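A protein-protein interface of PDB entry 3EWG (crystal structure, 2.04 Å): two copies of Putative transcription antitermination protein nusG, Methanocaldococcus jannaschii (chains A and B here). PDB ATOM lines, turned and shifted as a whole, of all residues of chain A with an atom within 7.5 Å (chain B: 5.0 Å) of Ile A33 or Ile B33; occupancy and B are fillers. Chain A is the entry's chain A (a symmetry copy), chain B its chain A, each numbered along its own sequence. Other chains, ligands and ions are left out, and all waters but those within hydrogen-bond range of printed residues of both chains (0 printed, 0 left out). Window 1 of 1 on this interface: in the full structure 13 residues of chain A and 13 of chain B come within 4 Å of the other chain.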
ATOM      1  N   GLU A  12     -27.387   3.357  26.622  1.00  0.00           N
ATOM      2  CA  GLU A  12     -27.031   1.970  26.299  1.00  0.00           C
ATOM      3  C   GLU A  12     -28.098   0.966  26.766  1.00  0.00           C
ATOM      4  O   GLU A  12     -28.575   0.152  25.973  1.00  0.00           O
ATOM      5  CB  GLU A  12     -25.648   1.611  26.867  1.00  0.00           C
ATOM      6  CG  GLU A  12     -24.501   2.540  26.425  1.00  0.00           C
ATOM      7  CD  GLU A  12     -24.394   3.811  27.265  1.00  0.00           C
ATOM      8  OE1 GLU A  12     -25.208   3.988  28.196  1.00  0.00           O
ATOM      9  OE2 GLU A  12     -23.490   4.633  27.007  1.00  0.00           O
ATOM     10  N   LYS A  13     -28.481   1.039  28.040  1.00  0.00           N
ATOM     11  CA  LYS A  13     -29.515   0.147  28.587  1.00  0.00           C
ATOM     12  C   LYS A  13     -30.897   0.388  27.965  1.00  0.00           C
ATOM     13  O   LYS A  13     -31.627  -0.563  27.668  1.00  0.00           O
ATOM     14  CB  LYS A  13     -29.592   0.272  30.110  1.00  0.00           C
ATOM     15  CG  LYS A  13     -28.458  -0.423  30.851  1.00  0.00           C
ATOM     16  CD  LYS A  13     -28.569  -0.196  32.346  1.00  0.00           C
ATOM     17  CE  LYS A  13     -27.948   1.133  32.750  1.00  0.00           C
ATOM     18  NZ  LYS A  13     -28.553   1.652  34.001  1.00  0.00           N
ATOM     19  N   ILE A  15     -31.583   1.507  24.954  1.00  0.00           N
ATOM     20  CA  ILE A  15     -31.573   0.986  23.588  1.00  0.00           C
ATOM     21  C   ILE A  15     -31.542  -0.550  23.566  1.00  0.00           C
ATOM     22  O   ILE A  15     -32.243  -1.169  22.769  1.00  0.00           O
ATOM     23  CB  ILE A  15     -30.444   1.634  22.749  1.00  0.00           C
ATOM     24  CG1 ILE A  15     -30.852   3.068  22.390  1.00  0.00           C
ATOM     25  CG2 ILE A  15     -30.165   0.837  21.464  1.00  0.00           C
ATOM     26  CD1 ILE A  15     -29.706   4.022  22.237  1.00  0.00           C
ATOM     27  N   ALA A  16     -30.760  -1.154  24.461  1.00  0.00           N
ATOM     28  CA  ALA A  16     -30.732  -2.612  24.607  1.00  0.00           C
ATOM     29  C   ALA A  16     -32.122  -3.181  24.904  1.00  0.00           C
ATOM     30  O   ALA A  16     -32.515  -4.196  24.328  1.00  0.00           O
ATOM     31  CB  ALA A  16     -29.741  -3.032  25.681  1.00  0.00           C
ATOM     32  N   GLY A  17     -32.854  -2.525  25.804  1.00  0.00           N
ATOM     33  CA  GLY A  17     -34.238  -2.888  26.104  1.00  0.00           C
ATOM     34  C   GLY A  17     -35.164  -2.811  24.903  1.00  0.00           C
ATOM     35  O   GLY A  17     -35.999  -3.700  24.689  1.00  0.00           O
ATOM     36  N   LEU A  18     -35.023  -1.742  24.120  1.00  0.00           N
ATOM     37  CA  LEU A  18     -35.808  -1.569  22.899  1.00  0.00           C
ATOM     38  C   LEU A  18     -35.432  -2.632  21.866  1.00  0.00           C
ATOM     39  O   LEU A  18     -36.304  -3.190  21.199  1.00  0.00           O
ATOM     40  CB  LEU A  18     -35.630  -0.157  22.315  1.00  0.00           C
ATOM     41  CG  LEU A  18     -36.015   1.093  23.123  1.00  0.00           C
ATOM     42  CD1 LEU A  18     -35.821   2.349  22.281  1.00  0.00           C
ATOM     43  CD2 LEU A  18     -37.450   1.038  23.668  1.00  0.00           C
ATOM     44  N   MET A  19     -34.131  -2.911  21.752  1.00  0.00           N
ATOM     45  CA  MET A  19     -33.615  -3.940  20.848  1.00  0.00           C
ATOM     46  C   MET A  19     -34.194  -5.326  21.121  1.00  0.00           C
ATOM     47  O   MET A  19     -34.658  -5.988  20.197  1.00  0.00           O
ATOM     48  CB  MET A  19     -32.093  -4.017  20.928  1.00  0.00           C
ATOM     49  CG  MET A  19     -31.365  -2.944  20.161  1.00  0.00           C
ATOM     50  SD  MET A  19     -29.619  -3.015  20.561  1.00  0.00           S
ATOM     51  CE  MET A  19     -28.986  -1.873  19.355  1.00  0.00           C
ATOM     52  N   ALA A  20     -34.146  -5.755  22.382  1.00  0.00           N
ATOM     53  CA  ALA A  20     -34.672  -7.062  22.794  1.00  0.00           C
ATOM     54  C   ALA A  20     -36.153  -7.211  22.465  1.00  0.00           C
ATOM     55  O   ALA A  20     -36.580  -8.247  21.955  1.00  0.00           O
ATOM     56  CB  ALA A  20     -34.423  -7.292  24.281  1.00  0.00           C
ATOM     57  N   SER A  21     -36.923  -6.161  22.750  1.00  0.00           N
ATOM     58  CA  SER A  21     -38.349  -6.111  22.439  1.00  0.00           C
ATOM     59  C   SER A  21     -38.609  -6.242  20.934  1.00  0.00           C
ATOM     60  O   SER A  21     -39.420  -7.065  20.514  1.00  0.00           O
ATOM     61  CB  SER A  21     -38.959  -4.812  22.977  1.00  0.00           C
ATOM     62  OG  SER A  21     -40.266  -4.602  22.470  1.00  0.00           O
ATOM     63  N   ALA A  23     -36.505  -7.296  18.537  1.00  0.00           N
ATOM     64  CA  ALA A  23     -35.943  -8.549  18.014  1.00  0.00           C
ATOM     65  C   ALA A  23     -36.920  -9.723  18.085  1.00  0.00           C
ATOM     66  O   ALA A  23     -37.062 -10.481  17.121  1.00  0.00           O
ATOM     67  CB  ALA A  23     -34.640  -8.901  18.735  1.00  0.00           C
ATOM     68  N   VAL A  30     -31.397 -12.124  15.978  1.00  0.00           N
ATOM     69  CA  VAL A  30     -30.519 -11.453  16.932  1.00  0.00           C
ATOM     70  C   VAL A  30     -30.378 -12.390  18.123  1.00  0.00           C
ATOM     71  O   VAL A  30     -31.374 -12.749  18.744  1.00  0.00           O
ATOM     72  CB  VAL A  30     -31.102 -10.082  17.354  1.00  0.00           C
ATOM     73  CG1 VAL A  30     -30.318  -9.478  18.513  1.00  0.00           C
ATOM     74  CG2 VAL A  30     -31.117  -9.124  16.163  1.00  0.00           C
ATOM     75  N   TYR A  31     -29.146 -12.788  18.426  1.00  0.00           N
ATOM     76  CA  TYR A  31     -28.899 -13.885  19.378  1.00  0.00           C
ATOM     77  C   TYR A  31     -28.476 -13.437  20.765  1.00  0.00           C
ATOM     78  O   TYR A  31     -28.824 -14.080  21.767  1.00  0.00           O
ATOM     79  CB  TYR A  31     -27.873 -14.878  18.814  1.00  0.00           C
ATOM     80  CG  TYR A  31     -28.195 -15.379  17.418  1.00  0.00           C
ATOM     81  CD1 TYR A  31     -29.457 -15.884  17.113  1.00  0.00           C
ATOM     82  CD2 TYR A  31     -27.231 -15.361  16.407  1.00  0.00           C
ATOM     83  CE1 TYR A  31     -29.762 -16.342  15.835  1.00  0.00           C
ATOM     84  CE2 TYR A  31     -27.526 -15.822  15.124  1.00  0.00           C
ATOM     85  CZ  TYR A  31     -28.799 -16.315  14.852  1.00  0.00           C
ATOM     86  OH  TYR A  31     -29.113 -16.780  13.599  1.00  0.00           O
ATOM     87  N   SER A  32     -27.712 -12.346  20.820  1.00  0.00           N
ATOM     88  CA  SER A  32     -27.181 -11.831  22.074  1.00  0.00           C
ATOM     89  C   SER A  32     -27.200 -10.306  22.100  1.00  0.00           C
ATOM     90  O   SER A  32     -27.060  -9.659  21.064  1.00  0.00           O
ATOM     91  CB  SER A  32     -25.749 -12.329  22.307  1.00  0.00           C
ATOM     92  OG  SER A  32     -25.638 -13.724  22.087  1.00  0.00           O
ATOM     93  N   ILE A  33     -27.385  -9.744  23.290  1.00  0.00           N
ATOM     94  CA  ILE A  33     -27.327  -8.296  23.491  1.00  0.00           C
ATOM     95  C   ILE A  33     -26.565  -8.013  24.784  1.00  0.00           C
ATOM     96  O   ILE A  33     -26.860  -8.615  25.821  1.00  0.00           O
ATOM     97  CB  ILE A  33     -28.741  -7.645  23.565  1.00  0.00           C
ATOM     98  CG1 ILE A  33     -29.530  -7.893  22.272  1.00  0.00           C
ATOM     99  CG2 ILE A  33     -28.632  -6.130  23.831  1.00  0.00           C
ATOM    100  CD1 ILE A  33     -31.015  -7.597  22.379  1.00  0.00           C
ATOM    101  N   LEU A  34     -25.580  -7.116  24.704  1.00  0.00           N
ATOM    102  CA  LEU A  34     -24.855  -6.626  25.882  1.00  0.00           C
ATOM    103  C   LEU A  34     -24.887  -5.103  25.981  1.00  0.00           C
ATOM    104  O   LEU A  34     -24.459  -4.395  25.061  1.00  0.00           O
ATOM    105  CB  LEU A  34     -23.398  -7.108  25.888  1.00  0.00           C
ATOM    106  CG  LEU A  34     -22.473  -6.498  26.959  1.00  0.00           C
ATOM    107  CD1 LEU A  34     -22.777  -7.045  28.338  1.00  0.00           C
ATOM    108  CD2 LEU A  34     -21.000  -6.695  26.619  1.00  0.00           C
ATOM    109  N   ALA A  35     -25.392  -4.607  27.108  1.00  0.00           N
ATOM    110  CA  ALA A  35     -25.300  -3.187  27.434  1.00  0.00           C
ATOM    111  C   ALA A  35     -24.606  -3.032  28.781  1.00  0.00           C
ATOM    112  O   ALA A  35     -24.855  -3.806  29.709  1.00  0.00           O
ATOM    113  CB  ALA A  35     -26.676  -2.549  27.465  1.00  0.00           C
ATOM    114  N   SER A  36     -23.729  -2.037  28.877  1.00  0.00           N
ATOM    115  CA  SER A  36     -22.979  -1.778  30.103  1.00  0.00           C
ATOM    116  C   SER A  36     -22.586  -0.311  30.211  1.00  0.00           C
ATOM    117  O   SER A  36     -22.094   0.285  29.246  1.00  0.00           O
ATOM    118  CB  SER A  36     -21.719  -2.647  30.156  1.00  0.00           C
ATOM    119  OG  SER A  36     -20.961  -2.363  31.321  1.00  0.00           O
ATOM    120  N   GLU A  37     -22.786   0.261  31.397  1.00  0.00           N
ATOM    121  CA  GLU A  37     -22.331   1.624  31.681  1.00  0.00           C
ATOM    122  C   GLU A  37     -20.816   1.750  31.529  1.00  0.00           C
ATOM    123  O   GLU A  37     -20.308   2.833  31.269  1.00  0.00           O
ATOM    124  CB  GLU A  37     -22.759   2.067  33.082  1.00  0.00           C
ATOM    125  CG  GLU A  37     -24.249   2.318  33.213  1.00  0.00           C
ATOM    126  CD  GLU A  37     -24.636   2.890  34.562  1.00  0.00           C
ATOM    127  OE1 GLU A  37     -23.742   3.312  35.330  1.00  0.00           O
ATOM    128  OE2 GLU A  37     -25.848   2.909  34.854  1.00  0.00           O
ATOM    129  N   VAL A  43     -23.729  -0.546  22.217  1.00  0.00           N
ATOM    130  CA  VAL A  43     -24.442  -1.764  22.585  1.00  0.00           C
ATOM    131  C   VAL A  43     -23.909  -2.860  21.664  1.00  0.00           C
ATOM    132  O   VAL A  43     -23.831  -2.680  20.440  1.00  0.00           O
ATOM    133  CB  VAL A  43     -25.985  -1.635  22.433  1.00  0.00           C
ATOM    134  CG1 VAL A  43     -26.691  -2.973  22.740  1.00  0.00           C
ATOM    135  CG2 VAL A  43     -26.536  -0.557  23.353  1.00  0.00           C
ATOM    136  N   LEU A  44     -23.517  -3.979  22.256  1.00  0.00           N
ATOM    137  CA  LEU A  44     -23.001  -5.099  21.478  1.00  0.00           C
ATOM    138  C   LEU A  44     -24.123  -6.066  21.167  1.00  0.00           C
ATOM    139  O   LEU A  44     -24.902  -6.434  22.054  1.00  0.00           O
ATOM    140  CB  LEU A  44     -21.845  -5.800  22.212  1.00  0.00           C
ATOM    141  CG  LEU A  44     -20.623  -4.931  22.551  1.00  0.00           C
ATOM    142  CD1 LEU A  44     -19.518  -5.762  23.192  1.00  0.00           C
ATOM    143  CD2 LEU A  44     -20.081  -4.188  21.325  1.00  0.00           C
ATOM    144  N   VAL A  45     -24.202  -6.454  19.893  1.00  0.00           N
ATOM    145  CA  VAL A  45     -25.279  -7.297  19.395  1.00  0.00           C
ATOM    146  C   VAL A  45     -24.698  -8.454  18.591  1.00  0.00           C
ATOM    147  O   VAL A  45     -23.967  -8.236  17.622  1.00  0.00           O
ATOM    148  CB  VAL A  45     -26.261  -6.494  18.497  1.00  0.00           C
ATOM    149  CG1 VAL A  45     -27.370  -7.397  17.948  1.00  0.00           C
ATOM    150  CG2 VAL A  45     -26.866  -5.324  19.259  1.00  0.00           C
ATOM    151  N   GLU A  46     -25.014  -9.678  19.004  1.00  0.00           N
ATOM    152  CA  GLU A  46     -24.724 -10.839  18.177  1.00  0.00           C
ATOM    153  C   GLU A  46     -25.920 -11.109  17.272  1.00  0.00           C
ATOM    154  O   GLU A  46     -27.059 -11.218  17.743  1.00  0.00           O
ATOM    155  CB  GLU A  46     -24.398 -12.074  19.018  1.00  0.00           C
ATOM    156  CG  GLU A  46     -23.852 -13.227  18.176  1.00  0.00           C
ATOM    157  CD  GLU A  46     -23.875 -14.572  18.874  1.00  0.00           C
ATOM    158  OE1 GLU A  46     -24.356 -14.670  20.029  1.00  0.00           O
ATOM    159  OE2 GLU A  46     -23.402 -15.543  18.252  1.00  0.00           O
ATOM    160  N   LEU A  56     -32.950  -3.999  13.131  1.00  0.00           N
ATOM    161  CA  LEU A  56     -33.106  -3.893  14.578  1.00  0.00           C
ATOM    162  C   LEU A  56     -33.084  -2.441  15.052  1.00  0.00           C
ATOM    163  O   LEU A  56     -33.881  -2.055  15.904  1.00  0.00           O
ATOM    164  CB  LEU A  56     -32.019  -4.714  15.293  1.00  0.00           C
ATOM    165  CG  LEU A  56     -31.971  -4.761  16.826  1.00  0.00           C
ATOM    166  CD1 LEU A  56     -33.122  -5.575  17.389  1.00  0.00           C
ATOM    167  CD2 LEU A  56     -30.642  -5.327  17.303  1.00  0.00           C
ATOM    168  N   LYS B  13     -33.638 -13.139  26.196  1.00  0.00           N
ATOM    169  CA  LYS B  13     -33.763 -11.814  25.568  1.00  0.00           C
ATOM    170  C   LYS B  13     -35.031 -11.067  26.005  1.00  0.00           C
ATOM    171  O   LYS B  13     -34.993  -9.858  26.253  1.00  0.00           O
ATOM    172  CB  LYS B  13     -33.715 -11.929  24.043  1.00  0.00           C
ATOM    173  CG  LYS B  13     -32.322 -12.175  23.479  1.00  0.00           C
ATOM    174  CD  LYS B  13     -32.371 -12.342  21.973  1.00  0.00           C
ATOM    175  CE  LYS B  13     -32.723 -13.772  21.587  1.00  0.00           C
ATOM    176  NZ  LYS B  13     -33.361 -13.828  20.250  1.00  0.00           N
ATOM    177  N   ALA B  16     -34.351  -9.830  29.566  1.00  0.00           N
ATOM    178  CA  ALA B  16     -33.362  -8.751  29.491  1.00  0.00           C
ATOM    179  C   ALA B  16     -33.996  -7.427  29.052  1.00  0.00           C
ATOM    180  O   ALA B  16     -33.698  -6.376  29.621  1.00  0.00           O
ATOM    181  CB  ALA B  16     -32.215  -9.127  28.567  1.00  0.00           C
ATOM    182  N   MET B  19     -36.062  -6.179  31.918  1.00  0.00           N
ATOM    183  CA  MET B  19     -35.114  -5.695  32.925  1.00  0.00           C
ATOM    184  C   MET B  19     -34.612  -4.281  32.647  1.00  0.00           C
ATOM    185  O   MET B  19     -34.641  -3.435  33.536  1.00  0.00           O
ATOM    186  CB  MET B  19     -33.916  -6.632  33.036  1.00  0.00           C
ATOM    187  CG  MET B  19     -34.164  -7.884  33.836  1.00  0.00           C
ATOM    188  SD  MET B  19     -32.762  -8.986  33.657  1.00  0.00           S
ATOM    189  CE  MET B  19     -33.181 -10.209  34.877  1.00  0.00           C
ATOM    190  N   ALA B  20     -34.141  -4.045  31.422  1.00  0.00           N
ATOM    191  CA  ALA B  20     -33.633  -2.732  31.009  1.00  0.00           C
ATOM    192  C   ALA B  20     -34.685  -1.638  31.160  1.00  0.00           C
ATOM    193  O   ALA B  20     -34.391  -0.552  31.660  1.00  0.00           O
ATOM    194  CB  ALA B  20     -33.114  -2.787  29.575  1.00  0.00           C
ATOM    195  N   VAL B  30     -28.717  -0.723  38.399  1.00  0.00           N
ATOM    196  CA  VAL B  30     -28.381  -1.847  37.529  1.00  0.00           C
ATOM    197  C   VAL B  30     -27.519  -1.283  36.409  1.00  0.00           C
ATOM    198  O   VAL B  30     -27.953  -0.390  35.688  1.00  0.00           O
ATOM    199  CB  VAL B  30     -29.658  -2.524  36.978  1.00  0.00           C
ATOM    200  CG1 VAL B  30     -29.324  -3.544  35.896  1.00  0.00           C
ATOM    201  CG2 VAL B  30     -30.440  -3.185  38.112  1.00  0.00           C
ATOM    202  N   TYR B  31     -26.299  -1.799  36.278  1.00  0.00           N
ATOM    203  CA  TYR B  31     -25.284  -1.173  35.414  1.00  0.00           C
ATOM    204  C   TYR B  31     -25.089  -1.851  34.070  1.00  0.00           C
ATOM    205  O   TYR B  31     -24.807  -1.183  33.064  1.00  0.00           O
ATOM    206  CB  TYR B  31     -23.937  -1.065  36.144  1.00  0.00           C
ATOM    207  CG  TYR B  31     -24.023  -0.412  37.512  1.00  0.00           C
ATOM    208  CD1 TYR B  31     -24.676   0.807  37.682  1.00  0.00           C
ATOM    209  CD2 TYR B  31     -23.437  -1.007  38.631  1.00  0.00           C
ATOM    210  CE1 TYR B  31     -24.761   1.411  38.933  1.00  0.00           C
ATOM    211  CE2 TYR B  31     -23.514  -0.407  39.888  1.00  0.00           C
ATOM    212  CZ  TYR B  31     -24.178   0.808  40.025  1.00  0.00           C
ATOM    213  OH  TYR B  31     -24.264   1.422  41.250  1.00  0.00           O
ATOM    214  N   SER B  32     -25.222  -3.177  34.059  1.00  0.00           N
ATOM    215  CA  SER B  32     -25.006  -3.970  32.858  1.00  0.00           C
ATOM    216  C   SER B  32     -26.011  -5.114  32.759  1.00  0.00           C
ATOM    217  O   SER B  32     -26.455  -5.648  33.775  1.00  0.00           O
ATOM    218  CB  SER B  32     -23.581  -4.538  32.825  1.00  0.00           C
ATOM    219  OG  SER B  32     -22.616  -3.544  33.120  1.00  0.00           O
ATOM    220  N   ILE B  33     -26.370  -5.473  31.532  1.00  0.00           N
ATOM    221  CA  ILE B  33     -27.246  -6.617  31.273  1.00  0.00           C
ATOM    222  C   ILE B  33     -26.701  -7.387  30.072  1.00  0.00           C
ATOM    223  O   ILE B  33     -26.403  -6.786  29.036  1.00  0.00           O
ATOM    224  CB  ILE B  33     -28.720  -6.191  30.997  1.00  0.00           C
ATOM    225  CG1 ILE B  33     -29.306  -5.430  32.194  1.00  0.00           C
ATOM    226  CG2 ILE B  33     -29.593  -7.421  30.678  1.00  0.00           C
ATOM    227  CD1 ILE B  33     -30.598  -4.690  31.893  1.00  0.00           C
ATOM    228  N   LEU B  34     -26.559  -8.704  30.231  1.00  0.00           N
ATOM    229  CA  LEU B  34     -26.191  -9.601  29.130  1.00  0.00           C
ATOM    230  C   LEU B  34     -27.196 -10.738  28.959  1.00  0.00           C
ATOM    231  O   LEU B  34     -27.450 -11.511  29.890  1.00  0.00           O
ATOM    232  CB  LEU B  34     -24.786 -10.187  29.324  1.00  0.00           C
ATOM    233  CG  LEU B  34     -24.360 -11.300  28.348  1.00  0.00           C
ATOM    234  CD1 LEU B  34     -24.062 -10.751  26.968  1.00  0.00           C
ATOM    235  CD2 LEU B  34     -23.171 -12.095  28.875  1.00  0.00           C
ATOM    236  N   ALA B  35     -27.759 -10.835  27.757  1.00  0.00           N
ATOM    237  CA  ALA B  35     -28.576 -11.985  27.380  1.00  0.00           C
ATOM    238  C   ALA B  35     -27.992 -12.616  26.121  1.00  0.00           C
ATOM    239  O   ALA B  35     -27.561 -11.910  25.207  1.00  0.00           O
ATOM    240  CB  ALA B  35     -30.018 -11.572  27.151  1.00  0.00           C
ATOM    241  N   VAL B  43     -29.760 -14.770  32.624  1.00  0.00           N
ATOM    242  CA  VAL B  43     -29.455 -13.400  32.228  1.00  0.00           C
ATOM    243  C   VAL B  43     -28.455 -12.876  33.256  1.00  0.00           C
ATOM    244  O   VAL B  43     -28.664 -13.007  34.471  1.00  0.00           O
ATOM    245  CB  VAL B  43     -30.713 -12.486  32.183  1.00  0.00           C
ATOM    246  CG1 VAL B  43     -30.331 -11.026  31.853  1.00  0.00           C
ATOM    247  CG2 VAL B  43     -31.716 -12.984  31.155  1.00  0.00           C
ATOM    248  N   LEU B  44     -27.360 -12.311  32.768  1.00  0.00           N
ATOM    249  CA  LEU B  44     -26.338 -11.765  33.654  1.00  0.00           C
ATOM    250  C   LEU B  44     -26.586 -10.287  33.868  1.00  0.00           C
ATOM    251  O   LEU B  44     -26.820  -9.541  32.911  1.00  0.00           O
ATOM    252  CB  LEU B  44     -24.926 -12.021  33.099  1.00  0.00           C
ATOM    253  CG  LEU B  44     -24.536 -13.491  32.873  1.00  0.00           C
ATOM    254  CD1 LEU B  44     -23.090 -13.611  32.411  1.00  0.00           C
ATOM    255  CD2 LEU B  44     -24.766 -14.350  34.120  1.00  0.00           C
ATOM    256  N   VAL B  45     -26.548  -9.883  35.138  1.00  0.00           N
ATOM    257  CA  VAL B  45     -26.865  -8.520  35.540  1.00  0.00           C
ATOM    258  C   VAL B  45     -25.776  -7.986  36.460  1.00  0.00           C
ATOM    259  O   VAL B  45     -25.488  -8.584  37.501  1.00  0.00           O
ATOM    260  CB  VAL B  45     -28.234  -8.447  36.273  1.00  0.00           C
ATOM    261  CG1 VAL B  45     -28.543  -7.015  36.723  1.00  0.00           C
ATOM    262  CG2 VAL B  45     -29.356  -8.973  35.391  1.00  0.00           C
ATOM    263  N   GLU B  46     -25.163  -6.873  36.068  1.00  0.00           N
ATOM    264  CA  GLU B  46     -24.292  -6.145  36.977  1.00  0.00           C
ATOM    265  C   GLU B  46     -25.121  -5.120  37.740  1.00  0.00           C
ATOM    266  O   GLU B  46     -25.845  -4.316  37.139  1.00  0.00           O
ATOM    267  CB  GLU B  46     -23.139  -5.461  36.239  1.00  0.00           C
ATOM    268  CG  GLU B  46     -22.082  -4.905  37.195  1.00  0.00           C
ATOM    269  CD  GLU B  46     -21.137  -3.904  36.560  1.00  0.00           C
ATOM    270  OE1 GLU B  46     -21.291  -3.570  35.360  1.00  0.00           O
ATOM    271  OE2 GLU B  46     -20.225  -3.449  37.280  1.00  0.00           O
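NZ of Lys B13 sits at hydrogen-bond distance from O of Val A30, 2.7 Å away.
O of Val B30 is in hydrogen-bond range of NZ of Lys A13.
O of Tyr B31 is in hydrogen-bond range of N of Glu A37 (3.0 Å).
The side-chain hydroxyl of Ser A36 sits at hydrogen-bond distance from the side-chain hydroxyl of Ser B32 (2.7 Å).
The backbone NH (N) of Ile B33 is in hydrogen-bond range of the backbone carbonyl oxygen (O) of Ala A35 (2.9 Å).
O of Ala B35 is in hydrogen-bond range of N of Ile A33, 2.9 Å away.
N of Tyr B31 lies within hydrogen-bond range of O of Glu B46, 2.7 Å away.
The side-chain hydroxyl (OG) of Ser B32 sits at hydrogen-bond distance from the side-chain carboxylate (OE1) of Glu B46 (2.6 Å).
The backbone NH (N) of Leu B34 is in hydrogen-bond range of the backbone carbonyl oxygen (O) of Leu B44 (2.8 Å).
The side-chain amino group (NZ) of Lys A13 is in salt-bridge range of the side-chain carboxylate (OE2) of Glu A37, at 3.1 Å.
OE1 of Glu A46 sits at hydrogen-bond distance from OG of Ser A32 (2.6 Å).
The backbone carbonyl oxygen (O) of Leu A44 sits at hydrogen-bond distance from the backbone NH (N) of Leu A34.
Among the printed residues, merely in contact across the chains: Lys A13 with Ala B20, Lys A13 with Tyr B31, Gly A17 with Ala B20, Ala A20 with Lys B13, Tyr A31 with Lys B13, Ser A32 with Ala B35, Ile A33 with Ile B33, Ile A33 with Leu B34, Leu A34 with Ile B33, Leu A34 with Leu B34, Ala A35 with Ser B32 and Ser A36 with Tyr B31.
Glu A12 touches none of the printed residues of chain B.
Of the printed residues of chain B, Ser A32 touches Ala B35 (3.2 Å).
Of chain B, only Ile B33, Leu B34 and Ala B35 come within 4 Å of Ile A33.
Printed residues of chain B within 4 Å of Ser A36: Tyr B31 (3.5 Å) and Ser B32 (2.7 Å).
Ile B33 touches three residues of chain A.
Printed residues of chain A within 4 Å of Ala B35: Ser A32 (3.2 Å) and Ile A33 (2.9 Å).
The nearest residue of chain B that does not touch Ile A33 is Lys B13 (4.9 Å).
Of the 23 printed residues of chain A, 11 touch a printed residue of chain B.
Hydrophobic or aromatic side chains of chain A within 4 Å of the printed part of chain B: Ala A20 and Leu A34.
Hydrophobic or aromatic side chains of chain B within 4 Å of the printed part of chain A: Ala B20, Tyr B31 and Leu B34.
Among the printed residues, no Asp or Glu carboxylate lies within 4 Å of a Lys or Arg side-chain nitrogen of the other chain.
Lys A13 touches Tyr B31, and with the chains exchanged Tyr A31 touches Lys B13.
Ile A33 touches its own counterpart, Ile B33.
Ile A33 touches Ala B35, and with the chains exchanged Ala A35 touches Ile B33.
Leu A34 touches its own counterpart, Leu B34.
Of the 18 pairs that touch across the chains among the printed residues, 14 have their exchanged pair printed and touching as well.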
